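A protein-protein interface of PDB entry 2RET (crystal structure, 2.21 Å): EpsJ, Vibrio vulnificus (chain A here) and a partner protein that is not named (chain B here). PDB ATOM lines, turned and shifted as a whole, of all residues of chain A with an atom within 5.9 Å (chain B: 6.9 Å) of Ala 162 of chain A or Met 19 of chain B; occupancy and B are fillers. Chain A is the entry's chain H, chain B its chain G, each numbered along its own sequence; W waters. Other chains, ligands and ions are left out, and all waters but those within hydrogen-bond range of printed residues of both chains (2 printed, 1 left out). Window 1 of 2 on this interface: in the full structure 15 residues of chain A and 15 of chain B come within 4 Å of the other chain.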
ATOM      1  N   LEU A  25     -17.854 -26.257 -22.645  1.00  0.00           N
ATOM      2  CA  LEU A  25     -16.760 -27.103 -23.023  1.00  0.00           C
ATOM      3  C   LEU A  25     -17.131 -28.161 -24.045  1.00  0.00           C
ATOM      4  O   LEU A  25     -16.303 -28.465 -24.898  1.00  0.00           O
ATOM      5  CB  LEU A  25     -16.158 -27.794 -21.809  1.00  0.00           C
ATOM      6  CG  LEU A  25     -15.326 -27.013 -20.799  1.00  0.00           C
ATOM      7  CD1 LEU A  25     -15.063 -27.960 -19.647  1.00  0.00           C
ATOM      8  CD2 LEU A  25     -14.023 -26.470 -21.389  1.00  0.00           C
ATOM      9  N   SER A 150      -4.082 -23.776 -28.102  1.00  0.00           N
ATOM     10  CA  SER A 150      -4.494 -23.739 -26.684  1.00  0.00           C
ATOM     11  C   SER A 150      -5.424 -22.577 -26.479  1.00  0.00           C
ATOM     12  O   SER A 150      -5.052 -21.449 -26.734  1.00  0.00           O
ATOM     13  CB  SER A 150      -3.292 -23.565 -25.760  1.00  0.00           C
ATOM     14  OG  SER A 150      -3.702 -23.502 -24.401  1.00  0.00           O
ATOM     15  N   VAL A 151      -6.627 -22.877 -26.021  1.00  0.00           N
ATOM     16  CA  VAL A 151      -7.664 -21.904 -25.752  1.00  0.00           C
ATOM     17  C   VAL A 151      -7.749 -21.768 -24.237  1.00  0.00           C
ATOM     18  O   VAL A 151      -8.057 -22.722 -23.549  1.00  0.00           O
ATOM     19  CB  VAL A 151      -9.035 -22.340 -26.335  1.00  0.00           C
ATOM     20  CG1 VAL A 151     -10.072 -21.211 -26.216  1.00  0.00           C
ATOM     21  CG2 VAL A 151      -8.885 -22.791 -27.840  1.00  0.00           C
ATOM     22  N   GLU A 152      -7.481 -20.558 -23.746  1.00  0.00           N
ATOM     23  CA  GLU A 152      -7.399 -20.256 -22.331  1.00  0.00           C
ATOM     24  C   GLU A 152      -8.533 -19.248 -21.985  1.00  0.00           C
ATOM     25  O   GLU A 152      -8.632 -18.163 -22.558  1.00  0.00           O
ATOM     26  CB  GLU A 152      -5.995 -19.692 -21.972  1.00  0.00           C
ATOM     27  CG  GLU A 152      -4.935 -19.751 -23.112  1.00  0.00           C
ATOM     28  CD  GLU A 152      -3.482 -19.794 -22.646  1.00  0.00           C
ATOM     29  OE1 GLU A 152      -2.940 -18.729 -22.256  1.00  0.00           O
ATOM     30  OE2 GLU A 152      -2.868 -20.904 -22.715  1.00  0.00           O
ATOM     31  N   LEU A 153      -9.418 -19.670 -21.092  1.00  0.00           N
ATOM     32  CA  LEU A 153     -10.491 -18.834 -20.530  1.00  0.00           C
ATOM     33  C   LEU A 153     -10.142 -18.498 -19.104  1.00  0.00           C
ATOM     34  O   LEU A 153      -9.727 -19.360 -18.368  1.00  0.00           O
ATOM     35  CB  LEU A 153     -11.827 -19.591 -20.525  1.00  0.00           C
ATOM     36  CG  LEU A 153     -12.429 -19.971 -21.874  1.00  0.00           C
ATOM     37  CD1 LEU A 153     -13.783 -20.601 -21.628  1.00  0.00           C
ATOM     38  CD2 LEU A 153     -12.555 -18.741 -22.742  1.00  0.00           C
ATOM     39  N   LYS A 160      -8.255 -19.455 -14.302  1.00  0.00           N
ATOM     40  CA  LYS A 160      -7.807 -19.844 -15.619  1.00  0.00           C
ATOM     41  C   LYS A 160      -8.030 -21.311 -15.857  1.00  0.00           C
ATOM     42  O   LYS A 160      -7.578 -22.130 -15.088  1.00  0.00           O
ATOM     43  CB  LYS A 160      -6.329 -19.471 -15.848  1.00  0.00           C
ATOM     44  CG  LYS A 160      -5.731 -20.088 -17.166  1.00  0.00           C
ATOM     45  CD  LYS A 160      -4.968 -19.068 -18.093  1.00  0.00           C
ATOM     46  CE  LYS A 160      -3.571 -18.699 -17.548  1.00  0.00           C
ATOM     47  NZ  LYS A 160      -2.631 -18.050 -18.572  1.00  0.00           N
ATOM     48  N   ILE A 161      -8.719 -21.621 -16.951  1.00  0.00           N
ATOM     49  CA  ILE A 161      -8.837 -22.978 -17.469  1.00  0.00           C
ATOM     50  C   ILE A 161      -8.435 -22.952 -18.965  1.00  0.00           C
ATOM     51  O   ILE A 161      -8.661 -21.965 -19.659  1.00  0.00           O
ATOM     52  CB  ILE A 161     -10.259 -23.569 -17.262  1.00  0.00           C
ATOM     53  CG1 ILE A 161     -11.318 -22.763 -18.038  1.00  0.00           C
ATOM     54  CG2 ILE A 161     -10.620 -23.591 -15.774  1.00  0.00           C
ATOM     55  CD1 ILE A 161     -12.677 -23.434 -18.119  1.00  0.00           C
ATOM     56  N   ALA A 162      -7.805 -24.031 -19.421  1.00  0.00           N
ATOM     57  CA  ALA A 162      -7.243 -24.128 -20.763  1.00  0.00           C
ATOM     58  C   ALA A 162      -7.551 -25.495 -21.402  1.00  0.00           C
ATOM     59  O   ALA A 162      -7.661 -26.524 -20.692  1.00  0.00           O
ATOM     60  CB  ALA A 162      -5.752 -23.887 -20.690  1.00  0.00           C
ATOM     61  N   ARG A 163      -7.753 -25.493 -22.728  1.00  0.00           N
ATOM     62  CA  ARG A 163      -7.880 -26.725 -23.496  1.00  0.00           C
ATOM     63  C   ARG A 163      -6.973 -26.656 -24.732  1.00  0.00           C
ATOM     64  O   ARG A 163      -6.945 -25.662 -25.468  1.00  0.00           O
ATOM     65  CB  ARG A 163      -9.346 -27.013 -23.873  1.00  0.00           C
ATOM     66  CG  ARG A 163     -10.194 -27.635 -22.726  1.00  0.00           C
ATOM     67  CD  ARG A 163      -9.828 -29.117 -22.428  1.00  0.00           C
ATOM     68  NE  ARG A 163     -10.241 -29.969 -23.543  1.00  0.00           N
ATOM     69  CZ  ARG A 163      -9.443 -30.571 -24.429  1.00  0.00           C
ATOM     70  NH1 ARG A 163      -8.115 -30.517 -24.366  1.00  0.00           N
ATOM     71  NH2 ARG A 163     -10.007 -31.271 -25.380  1.00  0.00           N
ATOM     72  N   THR A 164      -6.197 -27.722 -24.933  1.00  0.00           N
ATOM     73  CA  THR A 164      -5.265 -27.889 -26.045  1.00  0.00           C
ATOM     74  C   THR A 164      -5.937 -28.814 -27.058  1.00  0.00           C
ATOM     75  O   THR A 164      -6.402 -29.891 -26.695  1.00  0.00           O
ATOM     76  CB  THR A 164      -3.956 -28.540 -25.547  1.00  0.00           C
ATOM     77  OG1 THR A 164      -3.399 -27.737 -24.508  1.00  0.00           O
ATOM     78  CG2 THR A 164      -2.911 -28.746 -26.690  1.00  0.00           C
ATOM     79  N   GLN B  13     -13.877 -31.373  -9.352  1.00  0.00           N
ATOM     80  CA  GLN B  13     -12.646 -32.125  -9.439  1.00  0.00           C
ATOM     81  C   GLN B  13     -12.651 -33.074 -10.647  1.00  0.00           C
ATOM     82  O   GLN B  13     -11.691 -33.160 -11.367  1.00  0.00           O
ATOM     83  CB  GLN B  13     -12.402 -32.904  -8.150  1.00  0.00           C
ATOM     84  CG  GLN B  13     -12.254 -32.012  -6.924  1.00  0.00           C
ATOM     85  CD  GLN B  13     -10.862 -31.405  -6.751  1.00  0.00           C
ATOM     86  OE1 GLN B  13     -10.654 -30.189  -6.932  1.00  0.00           O
ATOM     87  NE2 GLN B  13      -9.911 -32.249  -6.360  1.00  0.00           N
ATOM     88  N   LYS B  14     -13.745 -33.782 -10.850  1.00  0.00           N
ATOM     89  CA  LYS B  14     -13.865 -34.724 -11.947  1.00  0.00           C
ATOM     90  C   LYS B  14     -13.669 -33.998 -13.308  1.00  0.00           C
ATOM     91  O   LYS B  14     -12.875 -34.411 -14.185  1.00  0.00           O
ATOM     92  CB  LYS B  14     -15.234 -35.373 -11.854  1.00  0.00           C
ATOM     93  CG  LYS B  14     -15.295 -36.811 -12.242  1.00  0.00           C
ATOM     94  CD  LYS B  14     -16.636 -37.405 -11.868  1.00  0.00           C
ATOM     95  CE  LYS B  14     -17.723 -37.057 -12.884  1.00  0.00           C
ATOM     96  NZ  LYS B  14     -17.933 -38.130 -13.922  1.00  0.00           N
ATOM     97  N   MET B  15     -14.366 -32.873 -13.437  1.00  0.00           N
ATOM     98  CA  MET B  15     -14.348 -32.090 -14.632  1.00  0.00           C
ATOM     99  C   MET B  15     -13.013 -31.432 -14.929  1.00  0.00           C
ATOM    100  O   MET B  15     -12.548 -31.470 -16.082  1.00  0.00           O
ATOM    101  CB  MET B  15     -15.414 -31.016 -14.536  1.00  0.00           C
ATOM    102  CG  MET B  15     -15.487 -30.116 -15.789  1.00  0.00           C
ATOM    103  SD  MET B  15     -16.902 -28.810 -15.582  1.00  0.00           S
ATOM    104  CE  MET B  15     -18.134 -29.897 -14.502  1.00  0.00           C
ATOM    105  N   PHE B  16     -12.403 -30.819 -13.910  1.00  0.00           N
ATOM    106  CA  PHE B  16     -11.106 -30.189 -14.104  1.00  0.00           C
ATOM    107  C   PHE B  16      -9.919 -31.198 -14.269  1.00  0.00           C
ATOM    108  O   PHE B  16      -9.010 -30.933 -15.058  1.00  0.00           O
ATOM    109  CB  PHE B  16     -10.816 -29.190 -13.000  1.00  0.00           C
ATOM    110  CG  PHE B  16     -11.844 -28.082 -12.876  1.00  0.00           C
ATOM    111  CD1 PHE B  16     -12.371 -27.461 -13.992  1.00  0.00           C
ATOM    112  CD2 PHE B  16     -12.258 -27.649 -11.618  1.00  0.00           C
ATOM    113  CE1 PHE B  16     -13.308 -26.434 -13.863  1.00  0.00           C
ATOM    114  CE2 PHE B  16     -13.192 -26.627 -11.482  1.00  0.00           C
ATOM    115  CZ  PHE B  16     -13.711 -26.015 -12.609  1.00  0.00           C
ATOM    116  N   ALA B  17      -9.919 -32.317 -13.537  1.00  0.00           N
ATOM    117  CA  ALA B  17      -8.935 -33.380 -13.763  1.00  0.00           C
ATOM    118  C   ALA B  17      -9.051 -33.935 -15.201  1.00  0.00           C
ATOM    119  O   ALA B  17      -8.023 -34.130 -15.866  1.00  0.00           O
ATOM    120  CB  ALA B  17      -9.061 -34.539 -12.687  1.00  0.00           C
ATOM    121  N   ALA B  18     -10.288 -34.108 -15.692  1.00  0.00           N
ATOM    122  CA  ALA B  18     -10.546 -34.562 -17.062  1.00  0.00           C
ATOM    123  C   ALA B  18     -10.003 -33.616 -18.115  1.00  0.00           C
ATOM    124  O   ALA B  18      -9.506 -34.081 -19.108  1.00  0.00           O
ATOM    125  CB  ALA B  18     -12.073 -34.861 -17.296  1.00  0.00           C
ATOM    126  N   MET B  19     -10.098 -32.300 -17.895  1.00  0.00           N
ATOM    127  CA  MET B  19      -9.512 -31.311 -18.786  1.00  0.00           C
ATOM    128  C   MET B  19      -7.988 -31.445 -18.864  1.00  0.00           C
ATOM    129  O   MET B  19      -7.432 -31.364 -19.906  1.00  0.00           O
ATOM    130  CB  MET B  19      -9.860 -29.895 -18.332  1.00  0.00           C
ATOM    131  CG  MET B  19     -11.339 -29.558 -18.470  1.00  0.00           C
ATOM    132  SD  MET B  19     -11.764 -27.725 -17.987  1.00  0.00           S
ATOM    133  CE  MET B  19     -10.792 -26.720 -19.342  1.00  0.00           C
ATOM    134  N   VAL B  20      -7.330 -31.612 -17.731  1.00  0.00           N
ATOM    135  CA  VAL B  20      -5.877 -31.814 -17.691  1.00  0.00           C
ATOM    136  C   VAL B  20      -5.480 -33.093 -18.468  1.00  0.00           C
ATOM    137  O   VAL B  20      -4.502 -33.065 -19.222  1.00  0.00           O
ATOM    138  CB  VAL B  20      -5.372 -31.851 -16.225  1.00  0.00           C
ATOM    139  CG1 VAL B  20      -3.848 -32.248 -16.114  1.00  0.00           C
ATOM    140  CG2 VAL B  20      -5.634 -30.524 -15.549  1.00  0.00           C
ATOM    141  N   ALA B  21      -6.235 -34.188 -18.270  1.00  0.00           N
ATOM    142  CA  ALA B  21      -6.013 -35.450 -18.981  1.00  0.00           C
ATOM    143  C   ALA B  21      -6.059 -35.232 -20.486  1.00  0.00           C
ATOM    144  O   ALA B  21      -5.158 -35.650 -21.167  1.00  0.00           O
ATOM    145  CB  ALA B  21      -7.044 -36.512 -18.571  1.00  0.00           C
ATOM    146  N   ASP B  22      -7.107 -34.571 -20.980  1.00  0.00           N
ATOM    147  CA  ASP B  22      -7.236 -34.202 -22.401  1.00  0.00           C
ATOM    148  C   ASP B  22      -6.057 -33.349 -22.893  1.00  0.00           C
ATOM    149  O   ASP B  22      -5.585 -33.533 -23.983  1.00  0.00           O
ATOM    150  CB  ASP B  22      -8.530 -33.420 -22.660  1.00  0.00           C
ATOM    151  CG  ASP B  22      -9.817 -34.278 -22.533  1.00  0.00           C
ATOM    152  OD1 ASP B  22      -9.774 -35.534 -22.672  1.00  0.00           O
ATOM    153  OD2 ASP B  22     -10.898 -33.655 -22.285  1.00  0.00           O
ATOM    154  N   ASN B  23      -5.612 -32.396 -22.092  1.00  0.00           N
ATOM    155  CA  ASN B  23      -4.493 -31.533 -22.481  1.00  0.00           C
ATOM    156  C   ASN B  23      -3.194 -32.297 -22.597  1.00  0.00           C
ATOM    157  O   ASN B  23      -2.373 -32.033 -23.488  1.00  0.00           O
ATOM    158  CB  ASN B  23      -4.314 -30.384 -21.477  1.00  0.00           C
ATOM    159  CG  ASN B  23      -5.465 -29.409 -21.504  1.00  0.00           C
ATOM    160  OD1 ASN B  23      -6.206 -29.356 -22.479  1.00  0.00           O
ATOM    161  ND2 ASN B  23      -5.619 -28.623 -20.436  1.00  0.00           N
ATOM    162  N   GLN B  24      -2.990 -33.233 -21.683  1.00  0.00           N
ATOM    163  CA  GLN B  24      -1.735 -33.971 -21.683  1.00  0.00           C
ATOM    164  C   GLN B  24      -1.767 -35.093 -22.724  1.00  0.00           C
ATOM    165  O   GLN B  24      -0.718 -35.458 -23.216  1.00  0.00           O
ATOM    166  CB  GLN B  24      -1.405 -34.493 -20.290  1.00  0.00           C
ATOM    167  CG  GLN B  24      -1.252 -33.378 -19.250  1.00  0.00           C
ATOM    168  CD  GLN B  24      -0.292 -32.309 -19.706  1.00  0.00           C
ATOM    169  OE1 GLN B  24       0.768 -32.599 -20.276  1.00  0.00           O
ATOM    170  NE2 GLN B  24      -0.659 -31.070 -19.480  1.00  0.00           N
ATOM    171  N   GLU B  42       0.086 -29.477 -13.821  1.00  0.00           N
ATOM    172  CA  GLU B  42      -0.651 -28.488 -14.610  1.00  0.00           C
ATOM    173  C   GLU B  42      -1.511 -27.687 -13.626  1.00  0.00           C
ATOM    174  O   GLU B  42      -2.243 -28.249 -12.842  1.00  0.00           O
ATOM    175  CB  GLU B  42      -1.539 -29.133 -15.686  1.00  0.00           C
ATOM    176  CG  GLU B  42      -2.246 -28.075 -16.607  1.00  0.00           C
ATOM    177  CD  GLU B  42      -2.945 -28.664 -17.830  1.00  0.00           C
ATOM    178  OE1 GLU B  42      -2.685 -29.849 -18.143  1.00  0.00           O
ATOM    179  OE2 GLU B  42      -3.750 -27.942 -18.486  1.00  0.00           O
ATOM    180  N   GLU B  43      -1.410 -26.378 -13.699  1.00  0.00           N
ATOM    181  CA  GLU B  43      -2.307 -25.513 -12.987  1.00  0.00           C
ATOM    182  C   GLU B  43      -3.584 -25.341 -13.800  1.00  0.00           C
ATOM    183  O   GLU B  43      -3.522 -24.961 -14.950  1.00  0.00           O
ATOM    184  CB  GLU B  43      -1.642 -24.157 -12.789  1.00  0.00           C
ATOM    185  CG  GLU B  43      -2.358 -23.275 -11.801  1.00  0.00           C
ATOM    186  CD  GLU B  43      -1.782 -23.375 -10.423  1.00  0.00           C
ATOM    187  OE1 GLU B  43      -0.824 -24.194 -10.219  1.00  0.00           O
ATOM    188  OE2 GLU B  43      -2.313 -22.622  -9.554  1.00  0.00           O
ATOM    189  N   LEU B  44      -4.732 -25.617 -13.189  1.00  0.00           N
ATOM    190  CA  LEU B  44      -6.038 -25.443 -13.847  1.00  0.00           C
ATOM    191  C   LEU B  44      -7.100 -25.151 -12.797  1.00  0.00           C
ATOM    192  O   LEU B  44      -7.226 -25.881 -11.808  1.00  0.00           O
ATOM    193  CB  LEU B  44      -6.402 -26.673 -14.680  1.00  0.00           C
ATOM    194  CG  LEU B  44      -7.604 -26.556 -15.635  1.00  0.00           C
ATOM    195  CD1 LEU B  44      -7.344 -27.286 -16.956  1.00  0.00           C
ATOM    196  CD2 LEU B  44      -8.911 -27.034 -14.982  1.00  0.00           C
ATOM    197  N   ALA B  45      -7.845 -24.064 -12.999  1.00  0.00           N
ATOM    198  CA  ALA B  45      -8.886 -23.642 -12.056  1.00  0.00           C
ATOM    199  C   ALA B  45      -8.343 -23.488 -10.637  1.00  0.00           C
ATOM    200  O   ALA B  45      -8.982 -23.905  -9.673  1.00  0.00           O
ATOM    201  CB  ALA B  45     -10.078 -24.594 -12.075  1.00  0.00           C
ATOM    202  N   VAL B  70      -4.366 -38.442 -13.835  1.00  0.00           N
ATOM    203  CA  VAL B  70      -4.335 -37.121 -13.185  1.00  0.00           C
ATOM    204  C   VAL B  70      -4.813 -37.230 -11.741  1.00  0.00           C
ATOM    205  O   VAL B  70      -5.925 -37.713 -11.469  1.00  0.00           O
ATOM    206  CB  VAL B  70      -5.248 -36.078 -13.936  1.00  0.00           C
ATOM    207  CG1 VAL B  70      -5.196 -34.708 -13.216  1.00  0.00           C
ATOM    208  CG2 VAL B  70      -4.818 -35.963 -15.426  1.00  0.00           C
ATOM    209  N   ILE B  80      -8.793 -39.463 -12.532  1.00  0.00           N
ATOM    210  CA  ILE B  80      -9.086 -39.866 -13.891  1.00  0.00           C
ATOM    211  C   ILE B  80      -7.884 -40.580 -14.543  1.00  0.00           C
ATOM    212  O   ILE B  80      -6.720 -40.209 -14.350  1.00  0.00           O
ATOM    213  CB  ILE B  80      -9.571 -38.613 -14.726  1.00  0.00           C
ATOM    214  CG1 ILE B  80      -9.909 -38.967 -16.183  1.00  0.00           C
ATOM    215  CG2 ILE B  80      -8.564 -37.500 -14.685  1.00  0.00           C
ATOM    216  CD1 ILE B  80     -11.084 -39.946 -16.291  1.00  0.00           C
HETATM  217  O   HOH W   1      -5.473 -21.895 -12.515  1.00  0.00           O
HETATM  218  O   HOH W   2      -1.460 -29.160 -23.355  1.00  0.00           O
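The side-chain carboxylate (OD2) of Asp 22 of chain B lies within salt-bridge range of the guanidinium group (NE) of Arg 163 of chain A, at 3.9 Å.
The backbone carbonyl oxygen (O) of Ala 162 of chain A lies within hydrogen-bond range of the side-chain amide nitrogen (ND2) of Asn 23 of chain B (2.9 Å).
OD1 of Asn 23 of chain B lies within hydrogen-bond range of NH1 of Arg 163 of chain A.
The side-chain amide oxygen (OD1) of Asn 23 of chain B is in hydrogen-bond range of the backbone NH (N) of Thr 164 of chain A (2.9 Å).
N of Ala 45 of chain B lies within hydrogen-bond range of O of Lys 160 of chain A.
The side-chain amide nitrogen (ND2) of Asn 23 of chain B sits close to the backbone carbonyl oxygen (O) of Met 19 of chain B (3.3 Å).
ND2 of Asn 23 of chain B lies within hydrogen-bond range of OE2 of Glu 42 of chain B, at 2.8 Å.
The backbone carbonyl oxygen (O) of Arg 163 of chain A is in hydrogen-bond range of the backbone NH (N) of Val 151 of chain A.
The side-chain carboxylate (OE1) of Glu 152 of chain A is in salt-bridge range of the side-chain amino group (NZ) of Lys 160 of chain A, at 3.8 Å.
O of Ile 161 of chain A lies within hydrogen-bond range of N of Leu 153 of chain A, 2.8 Å away.
Among the printed residues, merely in contact across the chains: Ala 162 of chain A with Met 19 of chain B, Arg 163 of chain A with Met 19 of chain B, Leu 25 of chain A with Met 19 of chain B, Ile 161 of chain A with Met 19 of chain B, Lys 160 of chain A with Leu 44 of chain B, Ala 162 of chain A with Leu 44 of chain B, Ile 161 of chain A with Ala 45 of chain B and Ile 161 of chain A with Leu 44 of chain B.
Of the printed residues of chain B, Ile 161 of chain A touches Met 19, Leu 44 and Ala 45.
Of the printed residues of chain B, Arg 163 of chain A touches Met 19, Asp 22 and Asn 23.
Of the printed residues of chain A, Met 19 of chain B touches Leu 25 (3.7 Å), Ile 161 (3.8 Å), Ala 162 (3.4 Å) and Arg 163 (3.6 Å).
Printed residues of chain A within 4 Å of Asp 22 of chain B: Arg 163.
Printed residues of chain A within 4 Å of Ala 45 of chain B: Lys 160 (2.9 Å) and Ile 161 (3.9 Å).
The nearest residue of chain B that does not touch Ala 162 of chain A is Glu 42 of chain B (4.7 Å).
The nearest printed residue of chain A that does not touch Met 19 of chain B is Thr 164 of chain A (6.3 Å).
Of the 10 printed residues of chain A, 6 touch a printed residue of chain B.
Of the 18 printed residues of chain B, 5 touch a printed residue of chain A.
Among the printed residues, 13 pairs touch across the chains.
Water W2 lies within hydrogen-bond range of OG1 of Thr 164 of chain A (2.7 Å) and O of Asn 23 of chain B (3.0 Å).
Water W1 bridges the backbone NH (N) of Ala 45 of chain B (3.3 Å) and the backbone carbonyl oxygen (O) of Lys 160 of chain A (3.3 Å).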
